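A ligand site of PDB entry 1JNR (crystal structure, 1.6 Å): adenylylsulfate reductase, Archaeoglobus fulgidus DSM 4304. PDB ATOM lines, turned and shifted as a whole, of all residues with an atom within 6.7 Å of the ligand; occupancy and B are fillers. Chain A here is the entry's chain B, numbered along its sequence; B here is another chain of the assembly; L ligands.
SG of Cys 47 is bound to FE2 of the ligand.
FE1 of the ligand is bound by SG of Cys 25, 2.4 Å away.
A sulfur (S1) of the ligand lies close to the backbone NH (N) of Cys 50.
The side-chain sulfur of Cys 50 is bound to an iron atom (FE3) of the ligand (2.4 Å).
The backbone NH (N) of Cys 53 lies close to a sulfur (S2) of the ligand (3.4 Å).
The side-chain sulfur (SG) of Cys 53 is bound to an iron atom (FE4) of the ligand, at 2.4 Å.
OG of Ser 3 sits close to S3 of the ligand, 3.2 Å away.
The backbone NH of Tyr 51 sits close to a sulfur (S1) of the ligand, at 3.4 Å.
ND2 of Asn 41 lies close to S3 of the ligand (3.5 Å).
N of Trp 48 lies close to S4 of the ligand (3.5 Å).
The backbone NH (N) of Ser 3 lies close to the side-chain sulfur (SG) of Cys 47, 3.6 Å away.
N of Glu 49 lies close to SG of Cys 47 (3.4 Å).
SG of Cys 25 sits close to N of Leu 29 (3.2 Å).
The side-chain sulfur of Cys 25 lies close to the backbone NH of Asn 27.
SG of Cys 25 lies close to N of Asp 28 (3.4 Å).
SG of Cys 50 lies close to OG of Ser 52, 3.2 Å away.
The side-chain amide nitrogen (ND2) of Asn 41 is in hydrogen-bond range of the side-chain hydroxyl (OG) of Ser 3 (3.0 Å).
The backbone nitrogen (N) of Pro 2 lies close to the side-chain carboxylate (OE2) of Glu 49 (2.6 Å).
The side-chain sulfur (SD) of Met 30 lies close to a sulfur (S3) of the ligand (3.7 Å).
Residues that only touch the ligand: Glu 49 (3.7 Å), Pro 26 (3.7 Å), Ser 52 (3.7 Å) and Leu 29 (3.98 Å).
Within 4 Å of the ligand: Ser 3, Cys 25, Pro 26, Leu 29, Met 30, Asn 41, Cys 47, Trp 48, Glu 49, Cys 50, Tyr 51, Ser 52 and Cys 53.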
ATOM      1  N   PRO A   2      11.224 -27.970  14.639  1.00  0.00           N
ATOM      2  CA  PRO A   2      12.373 -28.648  14.002  1.00  0.00           C
ATOM      3  C   PRO A   2      11.999 -30.035  13.514  1.00  0.00           C
ATOM      4  O   PRO A   2      10.998 -30.602  13.940  1.00  0.00           O
ATOM      5  CB  PRO A   2      13.479 -28.702  15.042  1.00  0.00           C
ATOM      6  CG  PRO A   2      13.160 -27.444  15.865  1.00  0.00           C
ATOM      7  CD  PRO A   2      11.629 -27.441  15.959  1.00  0.00           C
ATOM      8  N   SER A   3      12.817 -30.578  12.619  1.00  0.00           N
ATOM      9  CA  SER A   3      12.556 -31.912  12.079  1.00  0.00           C
ATOM     10  C   SER A   3      12.911 -32.973  13.106  1.00  0.00           C
ATOM     11  O   SER A   3      13.700 -32.734  14.017  1.00  0.00           O
ATOM     12  CB  SER A   3      13.389 -32.147  10.830  1.00  0.00           C
ATOM     13  OG  SER A   3      14.759 -32.320  11.183  1.00  0.00           O
ATOM     14  N   CYS A  21      18.269 -37.534   3.825  1.00  0.00           N
ATOM     15  CA  CYS A  21      18.200 -36.402   4.751  1.00  0.00           C
ATOM     16  C   CYS A  21      19.562 -35.766   5.007  1.00  0.00           C
ATOM     17  O   CYS A  21      19.690 -34.538   4.991  1.00  0.00           O
ATOM     18  CB  CYS A  21      17.549 -36.824   6.077  1.00  0.00           C
ATOM     19  SG  CYS A  21      18.376 -38.179   6.947  1.00  0.00           S
ATOM     20  N   ILE A  24      20.585 -33.766   1.832  1.00  0.00           N
ATOM     21  CA  ILE A  24      19.856 -32.555   1.480  1.00  0.00           C
ATOM     22  C   ILE A  24      19.876 -31.357   2.433  1.00  0.00           C
ATOM     23  O   ILE A  24      19.791 -30.211   1.985  1.00  0.00           O
ATOM     24  CB  ILE A  24      18.381 -32.904   1.163  1.00  0.00           C
ATOM     25  CG1 ILE A  24      17.772 -31.831   0.252  1.00  0.00           C
ATOM     26  CG2 ILE A  24      17.582 -33.051   2.446  1.00  0.00           C
ATOM     27  CD1 ILE A  24      18.330 -31.843  -1.162  1.00  0.00           C
ATOM     28  N   CYS A  25      19.986 -31.605   3.739  1.00  0.00           N
ATOM     29  CA  CYS A  25      19.945 -30.504   4.714  1.00  0.00           C
ATOM     30  C   CYS A  25      20.883 -29.335   4.490  1.00  0.00           C
ATOM     31  O   CYS A  25      22.101 -29.466   4.572  1.00  0.00           O
ATOM     32  CB  CYS A  25      20.161 -31.041   6.131  1.00  0.00           C
ATOM     33  SG  CYS A  25      20.027 -29.724   7.363  1.00  0.00           S
ATOM     34  N   PRO A  26      20.322 -28.143   4.224  1.00  0.00           N
ATOM     35  CA  PRO A  26      21.104 -26.927   3.973  1.00  0.00           C
ATOM     36  C   PRO A  26      21.940 -26.439   5.160  1.00  0.00           C
ATOM     37  O   PRO A  26      22.854 -25.631   4.985  1.00  0.00           O
ATOM     38  CB  PRO A  26      20.046 -25.907   3.573  1.00  0.00           C
ATOM     39  CG  PRO A  26      18.928 -26.757   3.016  1.00  0.00           C
ATOM     40  CD  PRO A  26      18.890 -27.895   3.986  1.00  0.00           C
ATOM     41  N   ASN A  27      21.641 -26.910   6.367  1.00  0.00           N
ATOM     42  CA  ASN A  27      22.397 -26.496   7.540  1.00  0.00           C
ATOM     43  C   ASN A  27      23.183 -27.635   8.206  1.00  0.00           C
ATOM     44  O   ASN A  27      23.632 -27.500   9.340  1.00  0.00           O
ATOM     45  CB  ASN A  27      21.486 -25.814   8.566  1.00  0.00           C
ATOM     46  CG  ASN A  27      22.128 -24.578   9.193  1.00  0.00           C
ATOM     47  OD1 ASN A  27      23.104 -24.044   8.659  1.00  0.00           O
ATOM     48  ND2 ASN A  27      21.575 -24.110  10.308  1.00  0.00           N
ATOM     49  N   ASP A  28      23.324 -28.745   7.488  1.00  0.00           N
ATOM     50  CA  ASP A  28      24.074 -29.903   7.969  1.00  0.00           C
ATOM     51  C   ASP A  28      23.588 -30.443   9.317  1.00  0.00           C
ATOM     52  O   ASP A  28      24.394 -30.766  10.195  1.00  0.00           O
ATOM     53  CB  ASP A  28      25.567 -29.552   8.059  1.00  0.00           C
ATOM     54  CG  ASP A  28      26.442 -30.762   8.387  1.00  0.00           C
ATOM     55  OD1 ASP A  28      26.226 -31.824   7.775  1.00  0.00           O
ATOM     56  OD2 ASP A  28      27.346 -30.652   9.249  1.00  0.00           O
ATOM     57  N   LEU A  29      22.277 -30.568   9.473  1.00  0.00           N
ATOM     58  CA  LEU A  29      21.719 -31.051  10.739  1.00  0.00           C
ATOM     59  C   LEU A  29      21.406 -32.531  10.782  1.00  0.00           C
ATOM     60  O   LEU A  29      21.545 -33.171  11.823  1.00  0.00           O
ATOM     61  CB  LEU A  29      20.448 -30.267  11.080  1.00  0.00           C
ATOM     62  CG  LEU A  29      20.540 -28.743  11.062  1.00  0.00           C
ATOM     63  CD1 LEU A  29      19.217 -28.168  11.544  1.00  0.00           C
ATOM     64  CD2 LEU A  29      21.678 -28.274  11.957  1.00  0.00           C
ATOM     65  N   MET A  30      20.975 -33.088   9.652  1.00  0.00           N
ATOM     66  CA  MET A  30      20.623 -34.499   9.604  1.00  0.00           C
ATOM     67  C   MET A  30      21.851 -35.392   9.459  1.00  0.00           C
ATOM     68  O   MET A  30      22.711 -35.157   8.610  1.00  0.00           O
ATOM     69  CB  MET A  30      19.655 -34.770   8.448  1.00  0.00           C
ATOM     70  CG  MET A  30      18.396 -33.913   8.504  1.00  0.00           C
ATOM     71  SD  MET A  30      17.499 -34.059  10.073  1.00  0.00           S
ATOM     72  CE  MET A  30      17.079 -35.795  10.062  1.00  0.00           C
ATOM     73  N   ASN A  41      18.167 -35.296  13.948  1.00  0.00           N
ATOM     74  CA  ASN A  41      18.555 -33.908  13.773  1.00  0.00           C
ATOM     75  C   ASN A  41      19.565 -33.655  14.898  1.00  0.00           C
ATOM     76  O   ASN A  41      19.213 -33.708  16.078  1.00  0.00           O
ATOM     77  CB  ASN A  41      17.336 -33.002  13.911  1.00  0.00           C
ATOM     78  CG  ASN A  41      17.661 -31.565  13.644  1.00  0.00           C
ATOM     79  OD1 ASN A  41      18.697 -31.061  14.083  1.00  0.00           O
ATOM     80  ND2 ASN A  41      16.780 -30.881  12.918  1.00  0.00           N
ATOM     81  N   PRO A  44      18.762 -29.197  16.588  1.00  0.00           N
ATOM     82  CA  PRO A  44      17.444 -28.617  16.307  1.00  0.00           C
ATOM     83  C   PRO A  44      17.256 -27.102  16.405  1.00  0.00           C
ATOM     84  O   PRO A  44      16.414 -26.563  15.698  1.00  0.00           O
ATOM     85  CB  PRO A  44      16.517 -29.390  17.257  1.00  0.00           C
ATOM     86  CG  PRO A  44      17.404 -29.762  18.390  1.00  0.00           C
ATOM     87  CD  PRO A  44      18.683 -30.166  17.700  1.00  0.00           C
ATOM     88  N   MET A  46      19.015 -24.997  15.223  1.00  0.00           N
ATOM     89  CA  MET A  46      19.618 -24.452  14.011  1.00  0.00           C
ATOM     90  C   MET A  46      18.782 -24.898  12.808  1.00  0.00           C
ATOM     91  O   MET A  46      19.179 -24.708  11.668  1.00  0.00           O
ATOM     92  CB  MET A  46      21.057 -24.953  13.864  1.00  0.00           C
ATOM     93  CG  MET A  46      22.086 -24.101  14.593  1.00  0.00           C
ATOM     94  SD  MET A  46      22.231 -22.444  13.885  1.00  0.00           S
ATOM     95  CE  MET A  46      23.846 -21.938  14.511  1.00  0.00           C
ATOM     96  N   CYS A  47      17.630 -25.494  13.094  1.00  0.00           N
ATOM     97  CA  CYS A  47      16.725 -25.963  12.035  1.00  0.00           C
ATOM     98  C   CYS A  47      15.846 -24.812  11.572  1.00  0.00           C
ATOM     99  O   CYS A  47      15.203 -24.139  12.380  1.00  0.00           O
ATOM    100  CB  CYS A  47      15.848 -27.112  12.558  1.00  0.00           C
ATOM    101  SG  CYS A  47      14.670 -27.797  11.361  1.00  0.00           S
ATOM    102  N   TRP A  48      15.819 -24.596  10.258  1.00  0.00           N
ATOM    103  CA  TRP A  48      15.032 -23.519   9.659  1.00  0.00           C
ATOM    104  C   TRP A  48      13.600 -23.991   9.354  1.00  0.00           C
ATOM    105  O   TRP A  48      12.750 -23.202   8.947  1.00  0.00           O
ATOM    106  CB  TRP A  48      15.716 -23.073   8.369  1.00  0.00           C
ATOM    107  CG  TRP A  48      15.458 -21.639   7.957  1.00  0.00           C
ATOM    108  CD1 TRP A  48      15.506 -20.541   8.759  1.00  0.00           C
ATOM    109  CD2 TRP A  48      15.196 -21.161   6.633  1.00  0.00           C
ATOM    110  NE1 TRP A  48      15.297 -19.407   8.024  1.00  0.00           N
ATOM    111  CE2 TRP A  48      15.102 -19.749   6.710  1.00  0.00           C
ATOM    112  CE3 TRP A  48      15.028 -21.780   5.384  1.00  0.00           C
ATOM    113  CZ2 TRP A  48      14.850 -18.950   5.595  1.00  0.00           C
ATOM    114  CZ3 TRP A  48      14.779 -20.991   4.269  1.00  0.00           C
ATOM    115  CH2 TRP A  48      14.697 -19.584   4.381  1.00  0.00           C
ATOM    116  N   GLU A  49      13.358 -25.278   9.580  1.00  0.00           N
ATOM    117  CA  GLU A  49      12.059 -25.891   9.284  1.00  0.00           C
ATOM    118  C   GLU A  49      11.730 -25.656   7.816  1.00  0.00           C
ATOM    119  O   GLU A  49      10.620 -25.244   7.461  1.00  0.00           O
ATOM    120  CB  GLU A  49      10.946 -25.333  10.186  1.00  0.00           C
ATOM    121  CG  GLU A  49      11.006 -25.887  11.612  1.00  0.00           C
ATOM    122  CD  GLU A  49       9.739 -25.646  12.438  1.00  0.00           C
ATOM    123  OE1 GLU A  49       8.845 -24.897  11.980  1.00  0.00           O
ATOM    124  OE2 GLU A  49       9.649 -26.190  13.560  1.00  0.00           O
ATOM    125  N   CYS A  50      12.724 -25.927   6.958  1.00  0.00           N
ATOM    126  CA  CYS A  50      12.570 -25.753   5.512  1.00  0.00           C
ATOM    127  C   CYS A  50      11.894 -26.970   4.865  1.00  0.00           C
ATOM    128  O   CYS A  50      11.492 -26.906   3.704  1.00  0.00           O
ATOM    129  CB  CYS A  50      13.923 -25.506   4.853  1.00  0.00           C
ATOM    130  SG  CYS A  50      15.013 -26.966   4.728  1.00  0.00           S
ATOM    131  N   TYR A  51      11.780 -28.057   5.623  1.00  0.00           N
ATOM    132  CA  TYR A  51      11.170 -29.299   5.154  1.00  0.00           C
ATOM    133  C   TYR A  51      11.870 -30.032   4.019  1.00  0.00           C
ATOM    134  O   TYR A  51      11.298 -30.941   3.408  1.00  0.00           O
ATOM    135  CB  TYR A  51       9.700 -29.058   4.753  1.00  0.00           C
ATOM    136  CG  TYR A  51       8.748 -28.957   5.916  1.00  0.00           C
ATOM    137  CD1 TYR A  51       8.764 -27.849   6.762  1.00  0.00           C
ATOM    138  CD2 TYR A  51       7.811 -29.964   6.179  1.00  0.00           C
ATOM    139  CE1 TYR A  51       7.880 -27.755   7.841  1.00  0.00           C
ATOM    140  CE2 TYR A  51       6.922 -29.883   7.254  1.00  0.00           C
ATOM    141  CZ  TYR A  51       6.965 -28.765   8.079  1.00  0.00           C
ATOM    142  OH  TYR A  51       6.079 -28.662   9.126  1.00  0.00           O
ATOM    143  N   SER A  52      13.119 -29.667   3.719  1.00  0.00           N
ATOM    144  CA  SER A  52      13.838 -30.348   2.659  1.00  0.00           C
ATOM    145  C   SER A  52      14.007 -31.829   2.994  1.00  0.00           C
ATOM    146  O   SER A  52      13.755 -32.695   2.157  1.00  0.00           O
ATOM    147  CB  SER A  52      15.206 -29.689   2.432  1.00  0.00           C
ATOM    148  OG  SER A  52      15.055 -28.400   1.860  1.00  0.00           O
ATOM    149  N   CYS A  53      14.439 -32.116   4.215  1.00  0.00           N
ATOM    150  CA  CYS A  53      14.641 -33.496   4.656  1.00  0.00           C
ATOM    151  C   CYS A  53      13.323 -34.260   4.592  1.00  0.00           C
ATOM    152  O   CYS A  53      13.278 -35.403   4.126  1.00  0.00           O
ATOM    153  CB  CYS A  53      15.203 -33.525   6.077  1.00  0.00           C
ATOM    154  SG  CYS A  53      14.217 -32.642   7.300  1.00  0.00           S
ATOM    155  N   VAL A  54      12.258 -33.640   5.071  1.00  0.00           N
ATOM    156  CA  VAL A  54      10.939 -34.264   5.075  1.00  0.00           C
ATOM    157  C   VAL A  54      10.540 -34.687   3.662  1.00  0.00           C
ATOM    158  O   VAL A  54      10.113 -35.820   3.437  1.00  0.00           O
ATOM    159  CB  VAL A  54       9.865 -33.292   5.630  1.00  0.00           C
ATOM    160  CG1 VAL A  54       8.485 -33.910   5.519  1.00  0.00           C
ATOM    161  CG2 VAL A  54      10.177 -32.955   7.090  1.00  0.00           C
ATOM    162  N   ILE A  62      10.349 -38.659   8.205  1.00  0.00           N
ATOM    163  CA  ILE A  62      10.679 -37.403   8.855  1.00  0.00           C
ATOM    164  C   ILE A  62       9.475 -36.460   8.917  1.00  0.00           C
ATOM    165  O   ILE A  62       8.753 -36.289   7.946  1.00  0.00           O
ATOM    166  CB  ILE A  62      11.833 -36.688   8.115  1.00  0.00           C
ATOM    167  CG1 ILE A  62      13.031 -37.635   7.986  1.00  0.00           C
ATOM    168  CG2 ILE A  62      12.254 -35.437   8.891  1.00  0.00           C
ATOM    169  CD1 ILE A  62      14.222 -37.034   7.267  1.00  0.00           C
ATOM    170  N   VAL A  64       7.958 -32.661  11.154  1.00  0.00           N
ATOM    171  CA  VAL A  64       8.417 -31.451  11.812  1.00  0.00           C
ATOM    172  C   VAL A  64       7.484 -31.128  12.962  1.00  0.00           C
ATOM    173  O   VAL A  64       6.259 -31.131  12.799  1.00  0.00           O
ATOM    174  CB  VAL A  64       8.461 -30.257  10.829  1.00  0.00           C
ATOM    175  CG1 VAL A  64       8.660 -28.952  11.589  1.00  0.00           C
ATOM    176  CG2 VAL A  64       9.598 -30.444   9.837  1.00  0.00           C
ATOM    177  N   ALA B  67      15.659 -22.675  -0.082  1.00  0.00           N
ATOM    178  CA  ALA B  67      15.504 -24.075   0.299  1.00  0.00           C
ATOM    179  C   ALA B  67      14.052 -24.557   0.326  1.00  0.00           C
ATOM    180  O   ALA B  67      13.774 -25.690  -0.049  1.00  0.00           O
ATOM    181  CB  ALA B  67      16.144 -24.311   1.671  1.00  0.00           C
ATOM    182  N   ILE B 237      19.003 -18.831   7.554  1.00  0.00           N
ATOM    183  CA  ILE B 237      19.875 -19.155   8.677  1.00  0.00           C
ATOM    184  C   ILE B 237      21.170 -19.785   8.148  1.00  0.00           C
ATOM    185  O   ILE B 237      22.180 -19.809   8.840  1.00  0.00           O
ATOM    186  CB  ILE B 237      19.162 -20.123   9.657  1.00  0.00           C
ATOM    187  CG1 ILE B 237      20.000 -20.296  10.923  1.00  0.00           C
ATOM    188  CG2 ILE B 237      18.927 -21.483   8.986  1.00  0.00           C
ATOM    189  CD1 ILE B 237      19.272 -21.075  12.014  1.00  0.00           C
ATOM    190  N   PHE B 238      21.129 -20.269   6.904  1.00  0.00           N
ATOM    191  CA  PHE B 238      22.282 -20.913   6.282  1.00  0.00           C
ATOM    192  C   PHE B 238      23.375 -19.935   5.878  1.00  0.00           C
ATOM    193  O   PHE B 238      24.515 -20.339   5.640  1.00  0.00           O
ATOM    194  CB  PHE B 238      21.839 -21.680   5.040  1.00  0.00           C
ATOM    195  CG  PHE B 238      20.530 -22.404   5.207  1.00  0.00           C
ATOM    196  CD1 PHE B 238      19.456 -22.108   4.373  1.00  0.00           C
ATOM    197  CD2 PHE B 238      20.385 -23.368   6.190  1.00  0.00           C
ATOM    198  CE1 PHE B 238      18.232 -22.777   4.532  1.00  0.00           C
ATOM    199  CE2 PHE B 238      19.167 -24.035   6.362  1.00  0.00           C
ATOM    200  CZ  PHE B 238      18.095 -23.738   5.519  1.00  0.00           C
HETATM  201 FE1  LIG L   1      17.729 -29.322   7.738  1.00  0.00          FE
HETATM  202 FE2  LIG L   1      15.729 -28.551   9.401  1.00  0.00          FE
HETATM  203 FE3  LIG L   1      15.576 -28.116   6.730  1.00  0.00          FE
HETATM  204 FE4  LIG L   1      15.379 -30.601   7.681  1.00  0.00          FE
HETATM  205  S1  LIG L   1      13.893 -28.901   8.090  1.00  0.00           S
HETATM  206  S2  LIG L   1      16.465 -29.968   5.953  1.00  0.00           S
HETATM  207  S3  LIG L   1      16.754 -30.481   9.448  1.00  0.00           S
HETATM  208  S4  LIG L   1      17.026 -27.183   8.152  1.00  0.00           S
